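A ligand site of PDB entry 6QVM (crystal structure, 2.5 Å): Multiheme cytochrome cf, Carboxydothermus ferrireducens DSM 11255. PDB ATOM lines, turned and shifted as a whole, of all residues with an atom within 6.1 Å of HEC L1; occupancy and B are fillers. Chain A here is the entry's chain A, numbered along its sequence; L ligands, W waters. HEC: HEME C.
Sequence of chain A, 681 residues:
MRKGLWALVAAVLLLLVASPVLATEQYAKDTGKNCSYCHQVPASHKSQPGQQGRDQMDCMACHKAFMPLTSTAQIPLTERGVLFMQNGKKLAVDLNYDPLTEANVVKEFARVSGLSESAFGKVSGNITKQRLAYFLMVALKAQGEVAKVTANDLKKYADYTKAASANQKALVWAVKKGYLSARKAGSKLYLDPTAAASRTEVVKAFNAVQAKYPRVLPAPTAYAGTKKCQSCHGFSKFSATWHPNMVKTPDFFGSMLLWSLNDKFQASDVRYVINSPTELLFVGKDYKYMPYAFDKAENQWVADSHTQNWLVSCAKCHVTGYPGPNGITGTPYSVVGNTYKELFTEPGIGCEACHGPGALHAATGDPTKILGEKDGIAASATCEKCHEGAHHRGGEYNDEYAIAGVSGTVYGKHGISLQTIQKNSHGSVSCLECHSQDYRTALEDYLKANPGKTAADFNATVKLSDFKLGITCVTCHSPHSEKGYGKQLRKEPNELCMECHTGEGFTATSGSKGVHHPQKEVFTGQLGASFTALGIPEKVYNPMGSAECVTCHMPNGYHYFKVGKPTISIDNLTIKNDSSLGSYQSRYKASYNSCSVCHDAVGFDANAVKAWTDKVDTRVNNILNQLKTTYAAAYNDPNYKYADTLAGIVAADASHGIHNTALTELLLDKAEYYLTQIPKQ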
ATOM      1  N   THR A  24      15.172  -6.925 -11.705  1.00  0.00           N
ATOM      2  CA  THR A  24      15.251  -6.139 -10.479  1.00  0.00           C
ATOM      3  C   THR A  24      14.035  -5.239 -10.343  1.00  0.00           C
ATOM      4  O   THR A  24      13.244  -5.088 -11.271  1.00  0.00           O
ATOM      5  CB  THR A  24      16.508  -5.266 -10.429  1.00  0.00           C
ATOM      6  OG1 THR A  24      16.464  -4.305 -11.493  1.00  0.00           O
ATOM      7  CG2 THR A  24      17.769  -6.117 -10.571  1.00  0.00           C
ATOM      8  N   GLU A  25      13.874  -4.634  -9.158  1.00  0.00           N
ATOM      9  CA  GLU A  25      12.819  -3.645  -8.972  1.00  0.00           C
ATOM     10  C   GLU A  25      13.004  -2.465  -9.914  1.00  0.00           C
ATOM     11  O   GLU A  25      12.021  -1.866 -10.373  1.00  0.00           O
ATOM     12  CB  GLU A  25      12.803  -3.180  -7.524  1.00  0.00           C
ATOM     13  CG  GLU A  25      12.386  -4.270  -6.543  1.00  0.00           C
ATOM     14  CD  GLU A  25      12.676  -3.916  -5.094  1.00  0.00           C
ATOM     15  OE1 GLU A  25      13.794  -4.179  -4.614  1.00  0.00           O
ATOM     16  OE2 GLU A  25      11.752  -3.389  -4.418  1.00  0.00           O
ATOM     17  N   TYR A  27      14.325  -2.614 -13.026  1.00  0.00           N
ATOM     18  CA  TYR A  27      13.844  -3.046 -14.337  1.00  0.00           C
ATOM     19  C   TYR A  27      12.324  -3.111 -14.370  1.00  0.00           C
ATOM     20  O   TYR A  27      11.720  -2.947 -15.434  1.00  0.00           O
ATOM     21  CB  TYR A  27      14.440  -4.407 -14.703  1.00  0.00           C
ATOM     22  CG  TYR A  27      15.957  -4.461 -14.751  1.00  0.00           C
ATOM     23  CD1 TYR A  27      16.699  -3.313 -14.999  1.00  0.00           C
ATOM     24  CD2 TYR A  27      16.632  -5.652 -14.546  1.00  0.00           C
ATOM     25  CE1 TYR A  27      18.082  -3.358 -15.047  1.00  0.00           C
ATOM     26  CE2 TYR A  27      18.011  -5.703 -14.587  1.00  0.00           C
ATOM     27  CZ  TYR A  27      18.740  -4.562 -14.833  1.00  0.00           C
ATOM     28  OH  TYR A  27      20.119  -4.612 -14.874  1.00  0.00           O
ATOM     29  N   ALA A  28      11.695  -3.375 -13.219  1.00  0.00           N
ATOM     30  CA  ALA A  28      10.239  -3.371 -13.161  1.00  0.00           C
ATOM     31  C   ALA A  28       9.689  -1.973 -13.411  1.00  0.00           C
ATOM     32  O   ALA A  28       8.721  -1.813 -14.168  1.00  0.00           O
ATOM     33  CB  ALA A  28       9.781  -3.913 -11.812  1.00  0.00           C
ATOM     34  N   THR A  31      10.342  -0.885 -17.163  1.00  0.00           N
ATOM     35  CA  THR A  31       9.572  -1.603 -18.167  1.00  0.00           C
ATOM     36  C   THR A  31       8.077  -1.613 -17.905  1.00  0.00           C
ATOM     37  O   THR A  31       7.302  -1.874 -18.830  1.00  0.00           O
ATOM     38  CB  THR A  31      10.076  -3.047 -18.272  1.00  0.00           C
ATOM     39  OG1 THR A  31       9.881  -3.702 -17.004  1.00  0.00           O
ATOM     40  CG2 THR A  31      11.553  -3.074 -18.644  1.00  0.00           C
ATOM     41  N   LYS A  33       6.594  -3.803 -15.986  1.00  0.00           N
ATOM     42  CA  LYS A  33       6.230  -5.215 -16.012  1.00  0.00           C
ATOM     43  C   LYS A  33       6.253  -5.823 -14.610  1.00  0.00           C
ATOM     44  O   LYS A  33       7.005  -5.386 -13.740  1.00  0.00           O
ATOM     45  CB  LYS A  33       7.172  -6.007 -16.917  1.00  0.00           C
ATOM     46  CG  LYS A  33       7.083  -5.639 -18.392  1.00  0.00           C
ATOM     47  CD  LYS A  33       5.759  -6.077 -18.986  1.00  0.00           C
ATOM     48  CE  LYS A  33       5.588  -5.495 -20.381  1.00  0.00           C
ATOM     49  NZ  LYS A  33       4.313  -5.928 -21.013  1.00  0.00           N
ATOM     50  N   ASN A  34       5.407  -6.835 -14.412  1.00  0.00           N
ATOM     51  CA  ASN A  34       5.430  -7.601 -13.177  1.00  0.00           C
ATOM     52  C   ASN A  34       6.733  -8.375 -13.052  1.00  0.00           C
ATOM     53  O   ASN A  34       7.381  -8.716 -14.059  1.00  0.00           O
ATOM     54  CB  ASN A  34       4.256  -8.571 -13.131  1.00  0.00           C
ATOM     55  CG  ASN A  34       2.988  -7.923 -12.651  1.00  0.00           C
ATOM     56  OD1 ASN A  34       2.889  -6.694 -12.585  1.00  0.00           O
ATOM     57  ND2 ASN A  34       1.994  -8.738 -12.310  1.00  0.00           N
ATOM     58  N   CYS A  35       7.114  -8.679 -11.808  1.00  0.00           N
ATOM     59  CA  CYS A  35       8.262  -9.541 -11.562  1.00  0.00           C
ATOM     60  C   CYS A  35       8.114 -10.854 -12.309  1.00  0.00           C
ATOM     61  O   CYS A  35       9.055 -11.330 -12.950  1.00  0.00           O
ATOM     62  CB  CYS A  35       8.418  -9.804 -10.063  1.00  0.00           C
ATOM     63  SG  CYS A  35       8.307  -8.359  -9.009  1.00  0.00           S
ATOM     64  N   SER A  36       6.911 -11.433 -12.262  1.00  0.00           N
ATOM     65  CA  SER A  36       6.659 -12.731 -12.876  1.00  0.00           C
ATOM     66  C   SER A  36       6.794 -12.707 -14.399  1.00  0.00           C
ATOM     67  O   SER A  36       6.801 -13.769 -15.014  1.00  0.00           O
ATOM     68  CB  SER A  36       5.261 -13.214 -12.486  1.00  0.00           C
ATOM     69  OG  SER A  36       4.261 -12.456 -13.149  1.00  0.00           O
ATOM     70  N   TYR A  37       6.882 -11.519 -15.000  1.00  0.00           N
ATOM     71  CA  TYR A  37       7.076 -11.421 -16.446  1.00  0.00           C
ATOM     72  C   TYR A  37       8.469 -11.893 -16.840  1.00  0.00           C
ATOM     73  O   TYR A  37       8.639 -12.604 -17.838  1.00  0.00           O
ATOM     74  CB  TYR A  37       6.817  -9.984 -16.904  1.00  0.00           C
ATOM     75  CG  TYR A  37       6.837  -9.772 -18.401  1.00  0.00           C
ATOM     76  CD1 TYR A  37       5.760 -10.147 -19.196  1.00  0.00           C
ATOM     77  CD2 TYR A  37       7.930  -9.177 -19.028  1.00  0.00           C
ATOM     78  CE1 TYR A  37       5.781  -9.952 -20.565  1.00  0.00           C
ATOM     79  CE2 TYR A  37       7.955  -8.977 -20.404  1.00  0.00           C
ATOM     80  CZ  TYR A  37       6.870  -9.359 -21.168  1.00  0.00           C
ATOM     81  OH  TYR A  37       6.875  -9.163 -22.531  1.00  0.00           O
ATOM     82  N   CYS A  38       9.485 -11.539 -16.040  1.00  0.00           N
ATOM     83  CA  CYS A  38      10.869 -11.920 -16.312  1.00  0.00           C
ATOM     84  C   CYS A  38      11.412 -12.974 -15.361  1.00  0.00           C
ATOM     85  O   CYS A  38      12.404 -13.619 -15.701  1.00  0.00           O
ATOM     86  CB  CYS A  38      11.775 -10.685 -16.245  1.00  0.00           C
ATOM     87  SG  CYS A  38      11.343  -9.363 -17.396  1.00  0.00           S
ATOM     88  N   HIS A  39      10.801 -13.150 -14.199  1.00  0.00           N
ATOM     89  CA  HIS A  39      11.288 -14.107 -13.202  1.00  0.00           C
ATOM     90  C   HIS A  39      10.281 -15.229 -13.014  1.00  0.00           C
ATOM     91  O   HIS A  39       9.074 -15.012 -13.064  1.00  0.00           O
ATOM     92  CB  HIS A  39      11.539 -13.427 -11.851  1.00  0.00           C
ATOM     93  CG  HIS A  39      12.625 -12.396 -11.885  1.00  0.00           C
ATOM     94  ND1 HIS A  39      13.963 -12.721 -11.720  1.00  0.00           N
ATOM     95  CD2 HIS A  39      12.578 -11.053 -12.061  1.00  0.00           C
ATOM     96  CE1 HIS A  39      14.689 -11.622 -11.792  1.00  0.00           C
ATOM     97  NE2 HIS A  39      13.878 -10.595 -11.995  1.00  0.00           N
ATOM     98  N   CYS A  59       6.143  -8.872  -4.275  1.00  0.00           N
ATOM     99  CA  CYS A  59       7.057  -9.870  -3.725  1.00  0.00           C
ATOM    100  C   CYS A  59       7.782  -9.331  -2.510  1.00  0.00           C
ATOM    101  O   CYS A  59       7.805  -9.973  -1.443  1.00  0.00           O
ATOM    102  CB  CYS A  59       8.062 -10.314  -4.792  1.00  0.00           C
ATOM    103  SG  CYS A  59       7.372 -10.531  -6.429  1.00  0.00           S
ATOM    104  N   MET A  60       8.390  -8.150  -2.640  1.00  0.00           N
ATOM    105  CA  MET A  60       9.304  -7.648  -1.627  1.00  0.00           C
ATOM    106  C   MET A  60       8.604  -7.140  -0.378  1.00  0.00           C
ATOM    107  O   MET A  60       9.286  -6.900   0.617  1.00  0.00           O
ATOM    108  CB  MET A  60      10.175  -6.539  -2.223  1.00  0.00           C
ATOM    109  CG  MET A  60      10.913  -6.958  -3.492  1.00  0.00           C
ATOM    110  SD  MET A  60      12.046  -8.345  -3.265  1.00  0.00           S
ATOM    111  CE  MET A  60      13.609  -7.585  -3.704  1.00  0.00           C
ATOM    112  N   LEU A  69      14.664 -12.017  -1.440  1.00  0.00           N
ATOM    113  CA  LEU A  69      14.997 -12.362  -2.824  1.00  0.00           C
ATOM    114  C   LEU A  69      16.254 -11.595  -3.207  1.00  0.00           C
ATOM    115  O   LEU A  69      16.226 -10.368  -3.353  1.00  0.00           O
ATOM    116  CB  LEU A  69      13.833 -12.035  -3.754  1.00  0.00           C
ATOM    117  CG  LEU A  69      12.498 -12.683  -3.389  1.00  0.00           C
ATOM    118  CD1 LEU A  69      11.378 -12.145  -4.281  1.00  0.00           C
ATOM    119  CD2 LEU A  69      12.589 -14.202  -3.495  1.00  0.00           C
ATOM    120  N   THR A  70      17.362 -12.317  -3.361  1.00  0.00           N
ATOM    121  CA  THR A  70      18.652 -11.697  -3.619  1.00  0.00           C
ATOM    122  C   THR A  70      19.311 -12.183  -4.901  1.00  0.00           C
ATOM    123  O   THR A  70      20.317 -11.599  -5.306  1.00  0.00           O
ATOM    124  CB  THR A  70      19.628 -11.966  -2.456  1.00  0.00           C
ATOM    125  OG1 THR A  70      19.870 -13.375  -2.375  1.00  0.00           O
ATOM    126  CG2 THR A  70      19.056 -11.467  -1.142  1.00  0.00           C
ATOM    127  N   SER A  71      18.776 -13.210  -5.544  1.00  0.00           N
ATOM    128  CA  SER A  71      19.546 -13.911  -6.571  1.00  0.00           C
ATOM    129  C   SER A  71      18.602 -14.560  -7.564  1.00  0.00           C
ATOM    130  O   SER A  71      17.471 -14.931  -7.214  1.00  0.00           O
ATOM    131  CB  SER A  71      20.448 -14.967  -5.920  1.00  0.00           C
ATOM    132  OG  SER A  71      20.934 -15.890  -6.878  1.00  0.00           O
ATOM    133  N   THR A  72      19.073 -14.709  -8.797  1.00  0.00           N
ATOM    134  CA  THR A  72      18.349 -15.451  -9.809  1.00  0.00           C
ATOM    135  C   THR A  72      18.435 -16.959  -9.587  1.00  0.00           C
ATOM    136  O   THR A  72      17.808 -17.713 -10.344  1.00  0.00           O
ATOM    137  CB  THR A  72      18.857 -15.116 -11.210  1.00  0.00           C
ATOM    138  OG1 THR A  72      20.281 -15.110 -11.222  1.00  0.00           O
ATOM    139  CG2 THR A  72      18.340 -13.751 -11.649  1.00  0.00           C
ATOM    140  N   GLN A  74      17.174 -18.026  -6.792  1.00  0.00           N
ATOM    141  CA  GLN A  74      15.837 -18.132  -6.223  1.00  0.00           C
ATOM    142  C   GLN A  74      14.780 -17.901  -7.294  1.00  0.00           C
ATOM    143  O   GLN A  74      13.802 -18.641  -7.387  1.00  0.00           O
ATOM    144  CB  GLN A  74      15.664 -17.117  -5.083  1.00  0.00           C
ATOM    145  CG  GLN A  74      16.727 -17.166  -4.004  1.00  0.00           C
ATOM    146  CD  GLN A  74      16.681 -15.937  -3.112  1.00  0.00           C
ATOM    147  OE1 GLN A  74      17.134 -14.858  -3.494  1.00  0.00           O
ATOM    148  NE2 GLN A  74      16.111 -16.093  -1.925  1.00  0.00           N
ATOM    149  N   ILE A  75      14.957 -16.849  -8.091  1.00  0.00           N
ATOM    150  CA  ILE A  75      13.981 -16.470  -9.111  1.00  0.00           C
ATOM    151  C   ILE A  75      14.644 -16.514 -10.487  1.00  0.00           C
ATOM    152  O   ILE A  75      15.041 -15.459 -11.017  1.00  0.00           O
ATOM    153  CB  ILE A  75      13.373 -15.098  -8.801  1.00  0.00           C
ATOM    154  CG1 ILE A  75      14.448 -14.108  -8.342  1.00  0.00           C
ATOM    155  CG2 ILE A  75      12.303 -15.233  -7.740  1.00  0.00           C
ATOM    156  CD1 ILE A  75      13.976 -12.668  -8.320  1.00  0.00           C
ATOM    157  N   LEU A  77      15.224 -16.691 -14.584  1.00  0.00           N
ATOM    158  CA  LEU A  77      14.566 -15.888 -15.605  1.00  0.00           C
ATOM    159  C   LEU A  77      13.610 -16.740 -16.431  1.00  0.00           C
ATOM    160  O   LEU A  77      13.866 -17.907 -16.708  1.00  0.00           O
ATOM    161  CB  LEU A  77      15.611 -15.244 -16.513  1.00  0.00           C
ATOM    162  CG  LEU A  77      16.624 -14.323 -15.838  1.00  0.00           C
ATOM    163  CD1 LEU A  77      17.694 -13.892 -16.831  1.00  0.00           C
ATOM    164  CD2 LEU A  77      15.932 -13.114 -15.244  1.00  0.00           C
ATOM    165  N   ARG A  80      11.052 -14.475 -21.388  1.00  0.00           N
ATOM    166  CA  ARG A  80      10.997 -13.028 -21.557  1.00  0.00           C
ATOM    167  C   ARG A  80      12.155 -12.345 -20.835  1.00  0.00           C
ATOM    168  O   ARG A  80      12.707 -11.356 -21.329  1.00  0.00           O
ATOM    169  CB  ARG A  80       9.655 -12.480 -21.073  1.00  0.00           C
ATOM    170  CG  ARG A  80       8.487 -12.898 -21.940  1.00  0.00           C
ATOM    171  CD  ARG A  80       8.510 -12.168 -23.274  1.00  0.00           C
ATOM    172  NE  ARG A  80       7.826 -12.905 -24.330  1.00  0.00           N
ATOM    173  CZ  ARG A  80       7.834 -12.532 -25.607  1.00  0.00           C
ATOM    174  NH1 ARG A  80       8.479 -11.443 -25.970  1.00  0.00           N
ATOM    175  NH2 ARG A  80       7.196 -13.260 -26.517  1.00  0.00           N
ATOM    176  N   GLY A  81      12.524 -12.851 -19.659  1.00  0.00           N
ATOM    177  CA  GLY A  81      13.659 -12.279 -18.954  1.00  0.00           C
ATOM    178  C   GLY A  81      14.973 -12.509 -19.676  1.00  0.00           C
ATOM    179  O   GLY A  81      15.816 -11.612 -19.773  1.00  0.00           O
ATOM    180  N   VAL A  82      15.151 -13.729 -20.207  1.00  0.00           N
ATOM    181  CA  VAL A  82      16.321 -14.041 -21.021  1.00  0.00           C
ATOM    182  C   VAL A  82      16.410 -13.100 -22.206  1.00  0.00           C
ATOM    183  O   VAL A  82      17.440 -12.441 -22.427  1.00  0.00           O
ATOM    184  CB  VAL A  82      16.281 -15.508 -21.466  1.00  0.00           C
ATOM    185  CG1 VAL A  82      17.309 -15.747 -22.553  1.00  0.00           C
ATOM    186  CG2 VAL A  82      16.510 -16.440 -20.288  1.00  0.00           C
ATOM    187  N   PHE A  84      14.961 -10.208 -22.676  1.00  0.00           N
ATOM    188  CA  PHE A  84      15.241  -8.877 -22.146  1.00  0.00           C
ATOM    189  C   PHE A  84      16.745  -8.684 -21.951  1.00  0.00           C
ATOM    190  O   PHE A  84      17.323  -7.685 -22.396  1.00  0.00           O
ATOM    191  CB  PHE A  84      14.481  -8.674 -20.838  1.00  0.00           C
ATOM    192  CG  PHE A  84      14.846  -7.414 -20.094  1.00  0.00           C
ATOM    193  CD1 PHE A  84      14.284  -6.195 -20.437  1.00  0.00           C
ATOM    194  CD2 PHE A  84      15.737  -7.451 -19.032  1.00  0.00           C
ATOM    195  CE1 PHE A  84      14.617  -5.042 -19.753  1.00  0.00           C
ATOM    196  CE2 PHE A  84      16.075  -6.303 -18.336  1.00  0.00           C
ATOM    197  CZ  PHE A  84      15.505  -5.102 -18.698  1.00  0.00           C
ATOM    198  N   MET A  85      17.403  -9.654 -21.315  1.00  0.00           N
ATOM    199  CA  MET A  85      18.822  -9.501 -21.004  1.00  0.00           C
ATOM    200  C   MET A  85      19.681  -9.650 -22.255  1.00  0.00           C
ATOM    201  O   MET A  85      20.692  -8.953 -22.400  1.00  0.00           O
ATOM    202  CB  MET A  85      19.232 -10.508 -19.936  1.00  0.00           C
ATOM    203  CG  MET A  85      20.568 -10.183 -19.300  1.00  0.00           C
ATOM    204  SD  MET A  85      20.890 -11.153 -17.820  1.00  0.00           S
ATOM    205  CE  MET A  85      22.563 -10.632 -17.437  1.00  0.00           C
ATOM    206  N   LYS A  89      19.089  -5.447 -22.093  1.00  0.00           N
ATOM    207  CA  LYS A  89      18.107  -5.045 -21.089  1.00  0.00           C
ATOM    208  C   LYS A  89      17.069  -4.084 -21.682  1.00  0.00           C
ATOM    209  O   LYS A  89      16.767  -3.033 -21.132  1.00  0.00           O
ATOM    210  CB  LYS A  89      18.796  -4.464 -19.847  1.00  0.00           C
ATOM    211  CG  LYS A  89      19.980  -5.318 -19.420  1.00  0.00           C
ATOM    212  CD  LYS A  89      20.079  -5.495 -17.927  1.00  0.00           C
ATOM    213  CE  LYS A  89      21.488  -5.907 -17.526  1.00  0.00           C
ATOM    214  NZ  LYS A  89      21.513  -6.824 -16.353  1.00  0.00           N
ATOM    215  N   LEU A  91      13.084  -4.650 -23.647  1.00  0.00           N
ATOM    216  CA  LEU A  91      12.056  -5.666 -23.847  1.00  0.00           C
ATOM    217  C   LEU A  91      12.035  -6.151 -25.291  1.00  0.00           C
ATOM    218  O   LEU A  91      12.114  -5.367 -26.230  1.00  0.00           O
ATOM    219  CB  LEU A  91      10.692  -5.091 -23.480  1.00  0.00           C
ATOM    220  CG  LEU A  91      10.380  -4.834 -22.001  1.00  0.00           C
ATOM    221  CD1 LEU A  91       9.014  -4.178 -21.864  1.00  0.00           C
ATOM    222  CD2 LEU A  91      10.432  -6.141 -21.207  1.00  0.00           C
HETATM  223 FE   HEC L   1      14.499  -8.806 -11.775  1.00  0.00          FE
HETATM  224  CHA HEC L   1      17.788  -9.737 -11.419  1.00  0.00           C
HETATM  225  CHB HEC L   1      14.068  -9.025  -8.382  1.00  0.00           C
HETATM  226  CHC HEC L   1      11.267  -7.634 -12.118  1.00  0.00           C
HETATM  227  CHD HEC L   1      14.807  -8.895 -15.231  1.00  0.00           C
HETATM  228  NA  HEC L   1      15.699  -9.279 -10.201  1.00  0.00           N
HETATM  229  C1A HEC L   1      17.020  -9.675 -10.269  1.00  0.00           C
HETATM  230  C2A HEC L   1      17.467 -10.005  -8.937  1.00  0.00           C
HETATM  231  C3A HEC L   1      16.435  -9.819  -8.104  1.00  0.00           C
HETATM  232  C4A HEC L   1      15.307  -9.358  -8.880  1.00  0.00           C
HETATM  233  CMA HEC L   1      16.432 -10.039  -6.577  1.00  0.00           C
HETATM  234  CAA HEC L   1      18.898 -10.515  -8.587  1.00  0.00           C
HETATM  235  CBA HEC L   1      19.629  -9.495  -7.728  1.00  0.00           C
HETATM  236  CGA HEC L   1      20.154  -8.362  -8.571  1.00  0.00           C
HETATM  237  O1A HEC L   1      20.178  -7.210  -8.077  1.00  0.00           O
HETATM  238  O2A HEC L   1      20.547  -8.620  -9.739  1.00  0.00           O
HETATM  239  NB  HEC L   1      12.953  -8.408 -10.507  1.00  0.00           N
HETATM  240  C1B HEC L   1      13.011  -8.535  -9.123  1.00  0.00           C
HETATM  241  C2B HEC L   1      11.750  -8.063  -8.583  1.00  0.00           C
HETATM  242  C3B HEC L   1      10.977  -7.689  -9.618  1.00  0.00           C
HETATM  243  C4B HEC L   1      11.718  -7.883 -10.846  1.00  0.00           C
HETATM  244  CMB HEC L   1      11.419  -8.060  -7.080  1.00  0.00           C
HETATM  245  CAB HEC L   1       9.531  -7.125  -9.543  1.00  0.00           C
HETATM  246  CBB HEC L   1       9.480  -5.784  -8.774  1.00  0.00           C
HETATM  247  NC  HEC L   1      13.270  -8.386 -13.367  1.00  0.00           N
HETATM  248  C1C HEC L   1      11.987  -7.880 -13.288  1.00  0.00           C
HETATM  249  C2C HEC L   1      11.486  -7.645 -14.627  1.00  0.00           C
HETATM  250  C3C HEC L   1      12.487  -7.947 -15.500  1.00  0.00           C
HETATM  251  C4C HEC L   1      13.611  -8.442 -14.712  1.00  0.00           C
HETATM  252  CMC HEC L   1      10.109  -7.023 -14.955  1.00  0.00           C
HETATM  253  CAC HEC L   1      12.476  -7.884 -17.048  1.00  0.00           C
HETATM  254  CBC HEC L   1      12.163  -6.476 -17.617  1.00  0.00           C
HETATM  255  ND  HEC L   1      16.048  -9.254 -13.110  1.00  0.00           N
HETATM  256  C1D HEC L   1      15.936  -9.221 -14.502  1.00  0.00           C
HETATM  257  C2D HEC L   1      17.214  -9.557 -15.077  1.00  0.00           C
HETATM  258  C3D HEC L   1      18.137  -9.828 -13.889  1.00  0.00           C
HETATM  259  C4D HEC L   1      17.327  -9.607 -12.707  1.00  0.00           C
HETATM  260  CMD HEC L   1      17.569  -9.646 -16.580  1.00  0.00           C
HETATM  261  CAD HEC L   1      19.623 -10.215 -13.914  1.00  0.00           C
HETATM  262  CBD HEC L   1      20.422  -8.919 -13.970  1.00  0.00           C
HETATM  263  CGD HEC L   1      21.905  -9.198 -13.923  1.00  0.00           C
HETATM  264  O1D HEC L   1      22.335 -10.029 -13.082  1.00  0.00           O
HETATM  265  O2D HEC L   1      22.649  -8.571 -14.722  1.00  0.00           O
HETATM  266 FE   HEC L   2      25.810 -16.153 -17.015  1.00  0.00          FE
HETATM  267  CHA HEC L   2      26.112 -15.470 -13.664  1.00  0.00           C
HETATM  268  CHB HEC L   2      29.020 -17.388 -17.041  1.00  0.00           C
HETATM  269  CHC HEC L   2      25.423 -17.137 -20.289  1.00  0.00           C
HETATM  270  CHD HEC L   2      22.872 -14.392 -17.227  1.00  0.00           C
HETATM  271  NA  HEC L   2      27.296 -16.366 -15.630  1.00  0.00           N
HETATM  272  C1A HEC L   2      27.203 -16.039 -14.293  1.00  0.00           C
HETATM  273  C2A HEC L   2      28.449 -16.394 -13.660  1.00  0.00           C
HETATM  274  C3A HEC L   2      29.250 -16.923 -14.588  1.00  0.00           C
HETATM  275  C4A HEC L   2      28.544 -16.914 -15.847  1.00  0.00           C
HETATM  276  CMA HEC L   2      30.693 -17.451 -14.358  1.00  0.00           C
HETATM  277  CAA HEC L   2      28.777 -16.204 -12.165  1.00  0.00           C
HETATM  278  CBA HEC L   2      28.266 -17.446 -11.429  1.00  0.00           C
HETATM  279  CGA HEC L   2      28.544 -17.332  -9.952  1.00  0.00           C
HETATM  280  O1A HEC L   2      28.251 -16.255  -9.349  1.00  0.00           O
HETATM  281  O2A HEC L   2      29.038 -18.327  -9.372  1.00  0.00           O
HETATM  282  NB  HEC L   2      27.025 -17.049 -18.433  1.00  0.00           N
HETATM  283  C1B HEC L   2      28.247 -17.626 -18.171  1.00  0.00           C
HETATM  284  C2B HEC L   2      28.581 -18.512 -19.270  1.00  0.00           C
HETATM  285  C3B HEC L   2      27.585 -18.429 -20.186  1.00  0.00           C
HETATM  286  C4B HEC L   2      26.587 -17.506 -19.657  1.00  0.00           C
HETATM  287  CMB HEC L   2      29.884 -19.326 -19.373  1.00  0.00           C
HETATM  288  CAB HEC L   2      27.473 -19.168 -21.533  1.00  0.00           C
HETATM  289  CBB HEC L   2      27.245 -20.676 -21.294  1.00  0.00           C
HETATM  290  NC  HEC L   2      24.435 -15.807 -18.482  1.00  0.00           N
HETATM  291  C1C HEC L   2      24.456 -16.317 -19.768  1.00  0.00           C
HETATM  292  C2C HEC L   2      23.218 -15.971 -20.446  1.00  0.00           C
HETATM  293  C3C HEC L   2      22.533 -15.148 -19.624  1.00  0.00           C
HETATM  294  C4C HEC L   2      23.265 -15.056 -18.368  1.00  0.00           C
HETATM  295  CMC HEC L   2      22.913 -16.290 -21.932  1.00  0.00           C
HETATM  296  CAC HEC L   2      21.186 -14.440 -19.923  1.00  0.00           C
HETATM  297  CBC HEC L   2      20.076 -15.477 -20.158  1.00  0.00           C
HETATM  298  ND  HEC L   2      24.681 -15.088 -15.652  1.00  0.00           N
HETATM  299  C1D HEC L   2      23.472 -14.473 -15.975  1.00  0.00           C
HETATM  300  C2D HEC L   2      22.931 -13.884 -14.780  1.00  0.00           C
HETATM  301  C3D HEC L   2      23.922 -14.221 -13.663  1.00  0.00           C
HETATM  302  C4D HEC L   2      24.995 -14.965 -14.302  1.00  0.00           C
HETATM  303  CMD HEC L   2      21.603 -13.107 -14.651  1.00  0.00           C
HETATM  304  CAD HEC L   2      23.804 -13.826 -12.174  1.00  0.00           C
HETATM  305  CBD HEC L   2      24.260 -12.388 -12.019  1.00  0.00           C
HETATM  306  CGD HEC L   2      25.723 -12.316 -12.335  1.00  0.00           C
HETATM  307  O1D HEC L   2      26.532 -12.839 -11.523  1.00  0.00           O
HETATM  308  O2D HEC L   2      26.087 -11.726 -13.391  1.00  0.00           O
HETATM  309  O   HOH W   1      21.450 -10.844 -10.754  1.00  0.00           O
HETATM  310  O   HOH W   2      21.837  -6.326 -11.211  1.00  0.00           O
HETATM  311  O   HOH W   3      20.976  -4.865  -8.573  1.00  0.00           O
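The backbone nitrogen (N) of Thr 24 is bound to an iron atom (FE) of HEC L1 (2.0 Å).
A ring nitrogen (NE2) of His 39 binds an iron atom (FE) of HEC L1, 1.9 Å away.
A carbon (CAB) of HEC L1 is bonded to the side-chain sulfur of Cys 35, at 1.8 Å.
The side-chain sulfur (SG) of Cys 38 is covalently linked to a carbon (CAC) of HEC L1, at 1.9 Å.
The side-chain amino group of Lys 89 is in salt-bridge range of an oxygen (O2D) of HEC L1, 2.6 Å away.
O of Ala 28 is in hydrogen-bond range of N of Lys 33, 3.4 Å away.
The backbone carbonyl oxygen (O) of Ile 75 sits at hydrogen-bond distance from a ring nitrogen (ND1) of His 39, at 3.0 Å.
The side-chain amide oxygen (OE1) of Gln 74 sits at hydrogen-bond distance from the backbone NH (N) of Thr 70 (2.6 Å).
The backbone carbonyl oxygen (O) of Tyr 27 sits at hydrogen-bond distance from the side-chain hydroxyl (OG1) of Thr 31 (2.5 Å).
The side-chain amino group (NZ) of Lys 89 is in hydrogen-bond range of the side-chain hydroxyl (OH) of Tyr 27 (3.0 Å).
The side-chain hydroxyl (OG1) of Thr 31 lies close to the backbone NH (N) of Lys 33 (3.4 Å).
N of Tyr 27 is in hydrogen-bond range of OG1 of Thr 24, 3.1 Å away.
The backbone NH (N) of Lys 89 lies within hydrogen-bond range of the backbone carbonyl oxygen (O) of Phe 84 (2.9 Å).
Merely in contact with HEC L1: Leu 69 (3.2 Å), Thr 70 (3.3 Å), Asn 34 (3.3 Å), Met 85 (3.4 Å), Phe 84 (3.5 Å), Ala 28 (3.6 Å), Thr 31 (3.6 Å), Ile 75 (3.6 Å), Tyr 27 (3.6 Å), Lys 33 (3.7 Å), Leu 77 (3.8 Å), Met 60 (3.8 Å), Glu 25 (3.9 Å) and Leu 91 (3.9996 Å).
Hydrophobic or aromatic side chains within 4 Å of HEC L1: Tyr 27, Ala 28, His 39, Met 60, Ile 75, Leu 77, Phe 84, Met 85 and Leu 91.
Of the 28 residues printed, 19 come within 4 Å of HEC L1.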
